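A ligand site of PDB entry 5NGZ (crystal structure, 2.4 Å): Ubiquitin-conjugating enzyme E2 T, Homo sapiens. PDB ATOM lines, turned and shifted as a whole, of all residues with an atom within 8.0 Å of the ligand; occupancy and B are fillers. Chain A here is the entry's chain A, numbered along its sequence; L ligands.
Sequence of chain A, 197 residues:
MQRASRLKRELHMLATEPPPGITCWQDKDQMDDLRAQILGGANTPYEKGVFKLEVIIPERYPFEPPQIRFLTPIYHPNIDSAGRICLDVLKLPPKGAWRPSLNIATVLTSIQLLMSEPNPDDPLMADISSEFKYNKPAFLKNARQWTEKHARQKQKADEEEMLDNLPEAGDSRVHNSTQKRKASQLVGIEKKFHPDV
The backbone carbonyl oxygen of Asp 80 sits close to a sulfur (S1) of the ligand (3.3 Å). The backbone carbonyl oxygen of Ser 81 sits close to a nitrogen (N1) of the ligand (3.1 Å). Merely in contact with the ligand: Thr 72 (3.8 Å), Pro 73 (3.4 Å), Ala 82 (3.9 Å), Gly 83 (3.7 Å) and Trp 146 (3.2 Å). Hydrophobic or aromatic side chains within 4 Å of the ligand: Pro 73 and Trp 146. Within 4 Å of the ligand: Phe 70, Leu 71, Thr 72, Pro 73, Ile 74, Asp 80, Ser 81, Ala 82, Gly 83 and Trp 146.
The backbone NH (N) of Phe 70 lies within hydrogen-bond range of the backbone carbonyl oxygen (O) of Gly 83 (3.0 Å). O of Trp 146 lies within hydrogen-bond range of ND1 of His 150 (3.4 Å). OD1 of Asp 80 is in hydrogen-bond range of N of Gly 83, 3.1 Å away. OD1 of Asp 80 sits at hydrogen-bond distance from N of Ala 82, at 2.9 Å. OD2 of Asp 80 is in salt-bridge range of NH1 of Arg 84, 3.2 Å away. The backbone NH (N) of Leu 71 lies within hydrogen-bond range of the backbone carbonyl oxygen (O) of Lys 52 (2.9 Å). OG1 of Thr 72 sits at hydrogen-bond distance from N of Lys 52 (2.8 Å).
O of Phe 70 lies within hydrogen-bond range of N2 of the ligand, at 3.0 Å. The backbone carbonyl oxygen (O) of Leu 71 is in hydrogen-bond range of a nitrogen (N2) of the ligand (3.4 Å). S1 of the ligand lies close to N of Ile 74, 3.4 Å away.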
ATOM      1  N   LYS A  52      -2.730  -8.131  -3.114  1.00  0.00           N
ATOM      2  CA  LYS A  52      -1.867  -7.246  -3.875  1.00  0.00           C
ATOM      3  C   LYS A  52      -0.408  -7.379  -3.407  1.00  0.00           C
ATOM      4  O   LYS A  52      -0.150  -7.532  -2.191  1.00  0.00           O
ATOM      5  CB  LYS A  52      -2.350  -5.801  -3.714  1.00  0.00           C
ATOM      6  CG  LYS A  52      -1.981  -4.915  -4.885  1.00  0.00           C
ATOM      7  CD  LYS A  52      -2.272  -3.434  -4.624  1.00  0.00           C
ATOM      8  CE  LYS A  52      -2.013  -2.593  -5.876  1.00  0.00           C
ATOM      9  NZ  LYS A  52      -1.446  -1.252  -5.551  1.00  0.00           N
ATOM     10  N   ARG A  69       7.043  -8.556  -2.108  1.00  0.00           N
ATOM     11  CA  ARG A  69       6.416  -8.592  -0.789  1.00  0.00           C
ATOM     12  C   ARG A  69       4.911  -8.314  -0.891  1.00  0.00           C
ATOM     13  O   ARG A  69       4.479  -7.586  -1.796  1.00  0.00           O
ATOM     14  CB  ARG A  69       7.098  -7.603   0.152  1.00  0.00           C
ATOM     15  CG  ARG A  69       6.732  -6.136  -0.049  1.00  0.00           C
ATOM     16  CD  ARG A  69       7.698  -5.213   0.691  1.00  0.00           C
ATOM     17  NE  ARG A  69       7.489  -3.792   0.365  1.00  0.00           N
ATOM     18  CZ  ARG A  69       6.540  -3.003   0.877  1.00  0.00           C
ATOM     19  NH1 ARG A  69       5.646  -3.451   1.761  1.00  0.00           N
ATOM     20  NH2 ARG A  69       6.475  -1.723   0.486  1.00  0.00           N
ATOM     21  N   PHE A  70       4.135  -8.902   0.025  1.00  0.00           N
ATOM     22  CA  PHE A  70       2.674  -8.717   0.057  1.00  0.00           C
ATOM     23  C   PHE A  70       2.382  -7.320   0.607  1.00  0.00           C
ATOM     24  O   PHE A  70       3.001  -6.918   1.594  1.00  0.00           O
ATOM     25  CB  PHE A  70       1.973  -9.750   0.951  1.00  0.00           C
ATOM     26  CG  PHE A  70       1.754 -11.078   0.284  1.00  0.00           C
ATOM     27  CD1 PHE A  70       0.500 -11.443  -0.182  1.00  0.00           C
ATOM     28  CD2 PHE A  70       2.800 -11.994   0.161  1.00  0.00           C
ATOM     29  CE1 PHE A  70       0.291 -12.679  -0.776  1.00  0.00           C
ATOM     30  CE2 PHE A  70       2.602 -13.233  -0.440  1.00  0.00           C
ATOM     31  CZ  PHE A  70       1.343 -13.585  -0.906  1.00  0.00           C
ATOM     32  N   LEU A  71       1.479  -6.586  -0.042  1.00  0.00           N
ATOM     33  CA  LEU A  71       0.921  -5.337   0.515  1.00  0.00           C
ATOM     34  C   LEU A  71      -0.348  -5.616   1.312  1.00  0.00           C
ATOM     35  O   LEU A  71      -0.605  -4.970   2.314  1.00  0.00           O
ATOM     36  CB  LEU A  71       0.684  -4.308  -0.592  1.00  0.00           C
ATOM     37  CG  LEU A  71       1.913  -3.856  -1.379  1.00  0.00           C
ATOM     38  CD1 LEU A  71       1.565  -2.991  -2.580  1.00  0.00           C
ATOM     39  CD2 LEU A  71       2.886  -3.115  -0.482  1.00  0.00           C
ATOM     40  N   THR A  72      -1.136  -6.589   0.844  1.00  0.00           N
ATOM     41  CA  THR A  72      -2.346  -7.039   1.523  1.00  0.00           C
ATOM     42  C   THR A  72      -1.972  -8.019   2.634  1.00  0.00           C
ATOM     43  O   THR A  72      -1.300  -9.010   2.358  1.00  0.00           O
ATOM     44  CB  THR A  72      -3.258  -7.801   0.544  1.00  0.00           C
ATOM     45  OG1 THR A  72      -3.466  -6.985  -0.630  1.00  0.00           O
ATOM     46  CG2 THR A  72      -4.595  -8.152   1.195  1.00  0.00           C
ATOM     47  N   PRO A  73      -2.418  -7.755   3.892  1.00  0.00           N
ATOM     48  CA  PRO A  73      -2.104  -8.688   4.964  1.00  0.00           C
ATOM     49  C   PRO A  73      -2.599 -10.111   4.708  1.00  0.00           C
ATOM     50  O   PRO A  73      -3.664 -10.293   4.130  1.00  0.00           O
ATOM     51  CB  PRO A  73      -2.802  -8.063   6.174  1.00  0.00           C
ATOM     52  CG  PRO A  73      -2.785  -6.600   5.904  1.00  0.00           C
ATOM     53  CD  PRO A  73      -2.974  -6.490   4.420  1.00  0.00           C
ATOM     54  N   ILE A  74      -1.787 -11.087   5.114  1.00  0.00           N
ATOM     55  CA  ILE A  74      -2.074 -12.514   4.957  1.00  0.00           C
ATOM     56  C   ILE A  74      -1.498 -13.312   6.143  1.00  0.00           C
ATOM     57  O   ILE A  74      -0.412 -13.007   6.627  1.00  0.00           O
ATOM     58  CB  ILE A  74      -1.531 -13.063   3.617  1.00  0.00           C
ATOM     59  CG1 ILE A  74      -2.001 -14.500   3.376  1.00  0.00           C
ATOM     60  CG2 ILE A  74      -0.005 -12.969   3.558  1.00  0.00           C
ATOM     61  CD1 ILE A  74      -1.622 -15.046   2.010  1.00  0.00           C
ATOM     62  N   TYR A  75      -2.221 -14.347   6.569  1.00  0.00           N
ATOM     63  CA  TYR A  75      -1.901 -15.138   7.751  1.00  0.00           C
ATOM     64  C   TYR A  75      -1.380 -16.470   7.238  1.00  0.00           C
ATOM     65  O   TYR A  75      -2.162 -17.266   6.718  1.00  0.00           O
ATOM     66  CB  TYR A  75      -3.189 -15.305   8.587  1.00  0.00           C
ATOM     67  CG  TYR A  75      -3.064 -16.027   9.918  1.00  0.00           C
ATOM     68  CD1 TYR A  75      -2.890 -15.316  11.106  1.00  0.00           C
ATOM     69  CD2 TYR A  75      -3.193 -17.419   9.995  1.00  0.00           C
ATOM     70  CE1 TYR A  75      -2.799 -15.965  12.324  1.00  0.00           C
ATOM     71  CE2 TYR A  75      -3.106 -18.077  11.211  1.00  0.00           C
ATOM     72  CZ  TYR A  75      -2.905 -17.340  12.377  1.00  0.00           C
ATOM     73  OH  TYR A  75      -2.819 -17.975  13.595  1.00  0.00           O
ATOM     74  N   HIS A  76      -0.074 -16.684   7.365  1.00  0.00           N
ATOM     75  CA  HIS A  76       0.642 -17.761   6.656  1.00  0.00           C
ATOM     76  C   HIS A  76       1.997 -17.975   7.360  1.00  0.00           C
ATOM     77  O   HIS A  76       2.654 -17.001   7.737  1.00  0.00           O
ATOM     78  CB  HIS A  76       0.850 -17.329   5.173  1.00  0.00           C
ATOM     79  CG  HIS A  76       1.305 -18.432   4.258  1.00  0.00           C
ATOM     80  ND1 HIS A  76       2.611 -18.867   4.206  1.00  0.00           N
ATOM     81  CD2 HIS A  76       0.634 -19.185   3.345  1.00  0.00           C
ATOM     82  CE1 HIS A  76       2.726 -19.829   3.313  1.00  0.00           C
ATOM     83  NE2 HIS A  76       1.537 -20.041   2.775  1.00  0.00           N
ATOM     84  N   ILE A  79       5.133 -16.126   5.627  1.00  0.00           N
ATOM     85  CA  ILE A  79       5.007 -14.704   5.279  1.00  0.00           C
ATOM     86  C   ILE A  79       4.896 -13.895   6.569  1.00  0.00           C
ATOM     87  O   ILE A  79       4.093 -14.220   7.415  1.00  0.00           O
ATOM     88  CB  ILE A  79       3.767 -14.459   4.388  1.00  0.00           C
ATOM     89  CG1 ILE A  79       3.915 -15.247   3.078  1.00  0.00           C
ATOM     90  CG2 ILE A  79       3.587 -12.968   4.097  1.00  0.00           C
ATOM     91  CD1 ILE A  79       2.630 -15.434   2.316  1.00  0.00           C
ATOM     92  N   ASP A  80       5.709 -12.844   6.721  1.00  0.00           N
ATOM     93  CA  ASP A  80       5.710 -12.091   7.979  1.00  0.00           C
ATOM     94  C   ASP A  80       4.779 -10.883   7.952  1.00  0.00           C
ATOM     95  O   ASP A  80       4.174 -10.588   6.931  1.00  0.00           O
ATOM     96  CB  ASP A  80       7.145 -11.767   8.460  1.00  0.00           C
ATOM     97  CG  ASP A  80       7.801 -10.575   7.758  1.00  0.00           C
ATOM     98  OD1 ASP A  80       7.173  -9.874   6.930  1.00  0.00           O
ATOM     99  OD2 ASP A  80       8.995 -10.340   8.072  1.00  0.00           O
ATOM    100  N   SER A  81       4.674 -10.202   9.095  1.00  0.00           N
ATOM    101  CA  SER A  81       3.799  -9.040   9.272  1.00  0.00           C
ATOM    102  C   SER A  81       4.153  -7.801   8.425  1.00  0.00           C
ATOM    103  O   SER A  81       3.339  -6.879   8.332  1.00  0.00           O
ATOM    104  CB  SER A  81       3.736  -8.654  10.764  1.00  0.00           C
ATOM    105  OG  SER A  81       4.998  -8.825  11.410  1.00  0.00           O
ATOM    106  N   ALA A  82       5.339  -7.775   7.839  1.00  0.00           N
ATOM    107  CA  ALA A  82       5.715  -6.735   6.882  1.00  0.00           C
ATOM    108  C   ALA A  82       5.563  -7.175   5.429  1.00  0.00           C
ATOM    109  O   ALA A  82       5.898  -6.407   4.516  1.00  0.00           O
ATOM    110  CB  ALA A  82       7.151  -6.306   7.128  1.00  0.00           C
ATOM    111  N   GLY A  83       5.102  -8.406   5.202  1.00  0.00           N
ATOM    112  CA  GLY A  83       4.922  -8.942   3.836  1.00  0.00           C
ATOM    113  C   GLY A  83       6.082  -9.689   3.201  1.00  0.00           C
ATOM    114  O   GLY A  83       5.989 -10.072   2.036  1.00  0.00           O
ATOM    115  N   ARG A  84       7.172  -9.924   3.946  1.00  0.00           N
ATOM    116  CA  ARG A  84       8.340 -10.649   3.398  1.00  0.00           C
ATOM    117  C   ARG A  84       7.988 -12.120   3.221  1.00  0.00           C
ATOM    118  O   ARG A  84       7.330 -12.701   4.061  1.00  0.00           O
ATOM    119  CB  ARG A  84       9.548 -10.538   4.320  1.00  0.00           C
ATOM    120  CG  ARG A  84      10.139  -9.147   4.512  1.00  0.00           C
ATOM    121  CD  ARG A  84      11.027  -9.070   5.761  1.00  0.00           C
ATOM    122  NE  ARG A  84      12.277  -9.838   5.659  1.00  0.00           N
ATOM    123  CZ  ARG A  84      12.762 -10.720   6.538  1.00  0.00           C
ATOM    124  NH1 ARG A  84      12.151 -11.008   7.689  1.00  0.00           N
ATOM    125  NH2 ARG A  84      13.919 -11.322   6.279  1.00  0.00           N
ATOM    126  N   MET A 125       7.060 -17.088  10.728  1.00  0.00           N
ATOM    127  CA  MET A 125       6.155 -16.827  11.831  1.00  0.00           C
ATOM    128  C   MET A 125       6.034 -18.116  12.622  1.00  0.00           C
ATOM    129  O   MET A 125       5.305 -19.040  12.213  1.00  0.00           O
ATOM    130  CB  MET A 125       4.786 -16.382  11.283  1.00  0.00           C
ATOM    131  CG  MET A 125       4.857 -15.153  10.412  1.00  0.00           C
ATOM    132  SD  MET A 125       5.399 -13.703  11.331  1.00  0.00           S
ATOM    133  CE  MET A 125       3.854 -13.192  12.070  1.00  0.00           C
ATOM    134  N   ILE A 128       2.483 -19.100  14.139  1.00  0.00           N
ATOM    135  CA  ILE A 128       1.571 -19.552  13.071  1.00  0.00           C
ATOM    136  C   ILE A 128       2.004 -20.923  12.565  1.00  0.00           C
ATOM    137  O   ILE A 128       1.166 -21.793  12.355  1.00  0.00           O
ATOM    138  CB  ILE A 128       1.501 -18.552  11.896  1.00  0.00           C
ATOM    139  CG1 ILE A 128       0.940 -17.219  12.379  1.00  0.00           C
ATOM    140  CG2 ILE A 128       0.586 -19.086  10.797  1.00  0.00           C
ATOM    141  CD1 ILE A 128       1.095 -16.091  11.382  1.00  0.00           C
ATOM    142  N   TRP A 146      -8.732 -13.678   8.735  1.00  0.00           N
ATOM    143  CA  TRP A 146      -7.769 -12.690   8.223  1.00  0.00           C
ATOM    144  C   TRP A 146      -8.083 -12.317   6.781  1.00  0.00           C
ATOM    145  O   TRP A 146      -8.013 -11.140   6.420  1.00  0.00           O
ATOM    146  CB  TRP A 146      -6.311 -13.174   8.395  1.00  0.00           C
ATOM    147  CG  TRP A 146      -5.756 -12.706   9.684  1.00  0.00           C
ATOM    148  CD1 TRP A 146      -6.118 -13.141  10.937  1.00  0.00           C
ATOM    149  CD2 TRP A 146      -4.799 -11.666   9.889  1.00  0.00           C
ATOM    150  NE1 TRP A 146      -5.435 -12.438  11.898  1.00  0.00           N
ATOM    151  CE2 TRP A 146      -4.610 -11.534  11.286  1.00  0.00           C
ATOM    152  CE3 TRP A 146      -4.070 -10.841   9.019  1.00  0.00           C
ATOM    153  CZ2 TRP A 146      -3.727 -10.612  11.842  1.00  0.00           C
ATOM    154  CZ3 TRP A 146      -3.187  -9.920   9.575  1.00  0.00           C
ATOM    155  CH2 TRP A 146      -3.031  -9.807  10.973  1.00  0.00           C
ATOM    156  N   HIS A 150      -9.126  -8.324   5.662  1.00  0.00           N
ATOM    157  CA  HIS A 150      -8.129  -7.505   4.924  1.00  0.00           C
ATOM    158  C   HIS A 150      -8.101  -7.654   3.399  1.00  0.00           C
ATOM    159  O   HIS A 150      -7.634  -6.747   2.706  1.00  0.00           O
ATOM    160  CB  HIS A 150      -6.724  -7.793   5.445  1.00  0.00           C
ATOM    161  CG  HIS A 150      -6.523  -7.463   6.887  1.00  0.00           C
ATOM    162  ND1 HIS A 150      -6.714  -8.386   7.898  1.00  0.00           N
ATOM    163  CD2 HIS A 150      -6.115  -6.322   7.494  1.00  0.00           C
ATOM    164  CE1 HIS A 150      -6.442  -7.827   9.061  1.00  0.00           C
ATOM    165  NE2 HIS A 150      -6.075  -6.572   8.847  1.00  0.00           N
HETATM  166  N1  LIG L   1       0.819  -7.065   6.601  1.00  0.00           N
HETATM  167  C1  LIG L   1       0.506  -7.691   7.803  1.00  0.00           C
HETATM  168  C2  LIG L   1       0.121  -7.090   9.029  1.00  0.00           C
HETATM  169  C3  LIG L   1      -0.150  -7.872  10.130  1.00  0.00           C
HETATM  170  C4  LIG L   1      -0.015  -9.263  10.050  1.00  0.00           C
HETATM  171  C5  LIG L   1       0.354  -9.878   8.871  1.00  0.00           C
HETATM  172  C6  LIG L   1       0.617  -9.099   7.747  1.00  0.00           C
HETATM  173  S1  LIG L   1       1.136  -9.604   6.149  1.00  0.00           S
HETATM  174  C7  LIG L   1       1.153  -7.911   5.688  1.00  0.00           C
HETATM  175  C8  LIG L   1       1.523  -7.484   4.302  1.00  0.00           C
HETATM  176  N2  LIG L   1       1.975  -6.090   4.256  1.00  0.00           N
